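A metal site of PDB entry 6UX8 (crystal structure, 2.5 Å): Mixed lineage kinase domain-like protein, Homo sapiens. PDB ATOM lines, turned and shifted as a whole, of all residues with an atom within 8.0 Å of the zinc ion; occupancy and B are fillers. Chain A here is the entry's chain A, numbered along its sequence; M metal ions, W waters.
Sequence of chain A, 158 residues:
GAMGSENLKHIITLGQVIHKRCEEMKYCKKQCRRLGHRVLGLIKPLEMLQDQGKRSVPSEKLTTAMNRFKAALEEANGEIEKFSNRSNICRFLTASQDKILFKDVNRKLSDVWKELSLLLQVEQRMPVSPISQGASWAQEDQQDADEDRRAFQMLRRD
The guanidinium group (NE) of Arg 33 lies within salt-bridge range of the side-chain carboxylate (OE2) of Glu 23, 3.1 Å away. ND1 of His 37 sits at hydrogen-bond distance from O of Arg 33, 3.1 Å away.
The zinc ion is bound by OE1 of Glu 23 (2.0 Å), NE2 of His 37 (2.0 Å), NE2 of His 19 (2.0 Å) and water W1 (2.1 Å).
Of the 10 residues printed, 3 come within 4 Å of the zinc ion. The nearest printed residue that does not touch the zinc ion is Arg 33 (4.1 Å).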
ATOM      1  N   HIS A  19      22.504  -4.201  12.891  1.00  0.00           N
ATOM      2  CA  HIS A  19      21.569  -3.239  12.321  1.00  0.00           C
ATOM      3  C   HIS A  19      22.273  -1.969  11.849  1.00  0.00           C
ATOM      4  O   HIS A  19      21.909  -1.399  10.826  1.00  0.00           O
ATOM      5  CB  HIS A  19      20.476  -2.900  13.346  1.00  0.00           C
ATOM      6  CG  HIS A  19      19.586  -1.776  12.920  1.00  0.00           C
ATOM      7  ND1 HIS A  19      19.566  -0.557  13.574  1.00  0.00           N
ATOM      8  CD2 HIS A  19      18.707  -1.669  11.905  1.00  0.00           C
ATOM      9  CE1 HIS A  19      18.693   0.241  12.985  1.00  0.00           C
ATOM     10  NE2 HIS A  19      18.162  -0.410  11.966  1.00  0.00           N
ATOM     11  N   LYS A  20      23.282  -1.521  12.595  1.00  0.00           N
ATOM     12  CA  LYS A  20      24.002  -0.316  12.214  1.00  0.00           C
ATOM     13  C   LYS A  20      24.805  -0.537  10.934  1.00  0.00           C
ATOM     14  O   LYS A  20      24.922   0.369  10.104  1.00  0.00           O
ATOM     15  CB  LYS A  20      24.920   0.134  13.341  1.00  0.00           C
ATOM     16  N   CYS A  22      23.985  -2.660   8.510  1.00  0.00           N
ATOM     17  CA  CYS A  22      23.047  -2.771   7.387  1.00  0.00           C
ATOM     18  C   CYS A  22      22.653  -1.401   6.868  1.00  0.00           C
ATOM     19  O   CYS A  22      22.462  -1.224   5.650  1.00  0.00           O
ATOM     20  CB  CYS A  22      21.814  -3.563   7.812  1.00  0.00           C
ATOM     21  SG  CYS A  22      22.112  -5.325   8.096  1.00  0.00           S
ATOM     22  N   GLU A  23      22.522  -0.407   7.753  1.00  0.00           N
ATOM     23  CA  GLU A  23      22.192   0.942   7.322  1.00  0.00           C
ATOM     24  C   GLU A  23      23.325   1.574   6.530  1.00  0.00           C
ATOM     25  O   GLU A  23      23.079   2.476   5.724  1.00  0.00           O
ATOM     26  CB  GLU A  23      21.855   1.810   8.528  1.00  0.00           C
ATOM     27  CG  GLU A  23      20.749   1.271   9.425  1.00  0.00           C
ATOM     28  CD  GLU A  23      19.368   1.434   8.820  1.00  0.00           C
ATOM     29  OE1 GLU A  23      18.422   0.761   9.309  1.00  0.00           O
ATOM     30  OE2 GLU A  23      19.213   2.237   7.878  1.00  0.00           O
ATOM     31  N   CYS A  32      19.292  -5.345   2.844  1.00  0.00           N
ATOM     32  CA  CYS A  32      20.127  -5.100   4.016  1.00  0.00           C
ATOM     33  C   CYS A  32      19.304  -4.495   5.156  1.00  0.00           C
ATOM     34  O   CYS A  32      19.369  -4.973   6.296  1.00  0.00           O
ATOM     35  CB  CYS A  32      21.298  -4.188   3.659  1.00  0.00           C
ATOM     36  SG  CYS A  32      22.372  -4.845   2.369  1.00  0.00           S
ATOM     37  N   ARG A  33      18.529  -3.449   4.859  1.00  0.00           N
ATOM     38  CA  ARG A  33      17.702  -2.850   5.897  1.00  0.00           C
ATOM     39  C   ARG A  33      16.607  -3.799   6.371  1.00  0.00           C
ATOM     40  O   ARG A  33      16.126  -3.678   7.508  1.00  0.00           O
ATOM     41  CB  ARG A  33      17.096  -1.541   5.391  1.00  0.00           C
ATOM     42  CG  ARG A  33      18.115  -0.528   4.902  1.00  0.00           C
ATOM     43  CD  ARG A  33      17.474   0.778   4.479  1.00  0.00           C
ATOM     44  NE  ARG A  33      17.159   1.634   5.626  1.00  0.00           N
ATOM     45  CZ  ARG A  33      15.973   1.710   6.210  1.00  0.00           C
ATOM     46  NH1 ARG A  33      14.958   0.975   5.770  1.00  0.00           N
ATOM     47  NH2 ARG A  33      15.787   2.515   7.254  1.00  0.00           N
ATOM     48  N   ARG A  34      16.215  -4.754   5.520  1.00  0.00           N
ATOM     49  CA  ARG A  34      15.271  -5.778   5.947  1.00  0.00           C
ATOM     50  C   ARG A  34      15.911  -6.726   6.961  1.00  0.00           C
ATOM     51  O   ARG A  34      15.265  -7.116   7.938  1.00  0.00           O
ATOM     52  CB  ARG A  34      14.760  -6.562   4.737  1.00  0.00           C
ATOM     53  CG  ARG A  34      13.770  -7.668   5.068  1.00  0.00           C
ATOM     54  CD  ARG A  34      12.380  -7.110   5.320  1.00  0.00           C
ATOM     55  NE  ARG A  34      11.823  -6.510   4.111  1.00  0.00           N
ATOM     56  CZ  ARG A  34      10.601  -6.000   4.034  1.00  0.00           C
ATOM     57  NH1 ARG A  34       9.801  -6.010   5.100  1.00  0.00           N
ATOM     58  NH2 ARG A  34      10.171  -5.469   2.898  1.00  0.00           N
ATOM     59  N   GLY A  36      18.640  -6.099   8.992  1.00  0.00           N
ATOM     60  CA  GLY A  36      18.937  -5.412  10.236  1.00  0.00           C
ATOM     61  C   GLY A  36      17.716  -5.135  11.084  1.00  0.00           C
ATOM     62  O   GLY A  36      17.791  -5.153  12.317  1.00  0.00           O
ATOM     63  N   HIS A  37      16.569  -4.882  10.443  1.00  0.00           N
ATOM     64  CA  HIS A  37      15.347  -4.633  11.189  1.00  0.00           C
ATOM     65  C   HIS A  37      14.728  -5.922  11.718  1.00  0.00           C
ATOM     66  O   HIS A  37      14.053  -5.901  12.755  1.00  0.00           O
ATOM     67  CB  HIS A  37      14.338  -3.873  10.316  1.00  0.00           C
ATOM     68  CG  HIS A  37      14.752  -2.464  10.027  1.00  0.00           C
ATOM     69  ND1 HIS A  37      14.253  -1.745   8.959  1.00  0.00           N
ATOM     70  CD2 HIS A  37      15.606  -1.636  10.674  1.00  0.00           C
ATOM     71  CE1 HIS A  37      14.784  -0.543   8.955  1.00  0.00           C
ATOM     72  NE2 HIS A  37      15.617  -0.448   9.986  1.00  0.00           N
ATOM     73  N   LEU A  40      16.639  -6.523  14.859  1.00  0.00           N
ATOM     74  CA  LEU A  40      16.126  -5.669  15.922  1.00  0.00           C
ATOM     75  C   LEU A  40      14.870  -6.264  16.551  1.00  0.00           C
ATOM     76  O   LEU A  40      14.663  -6.170  17.766  1.00  0.00           O
ATOM     77  CB  LEU A  40      15.843  -4.261  15.397  1.00  0.00           C
ATOM     78  CG  LEU A  40      17.039  -3.388  15.042  1.00  0.00           C
ATOM     79  CD1 LEU A  40      16.566  -2.007  14.635  1.00  0.00           C
ATOM     80  CD2 LEU A  40      18.005  -3.305  16.209  1.00  0.00           C
HETATM   81 ZN    ZN M   1      17.046   0.783  10.749  1.00  0.00          ZN
HETATM   82  O   HOH W   1      16.906   2.807  11.244  1.00  0.00           O
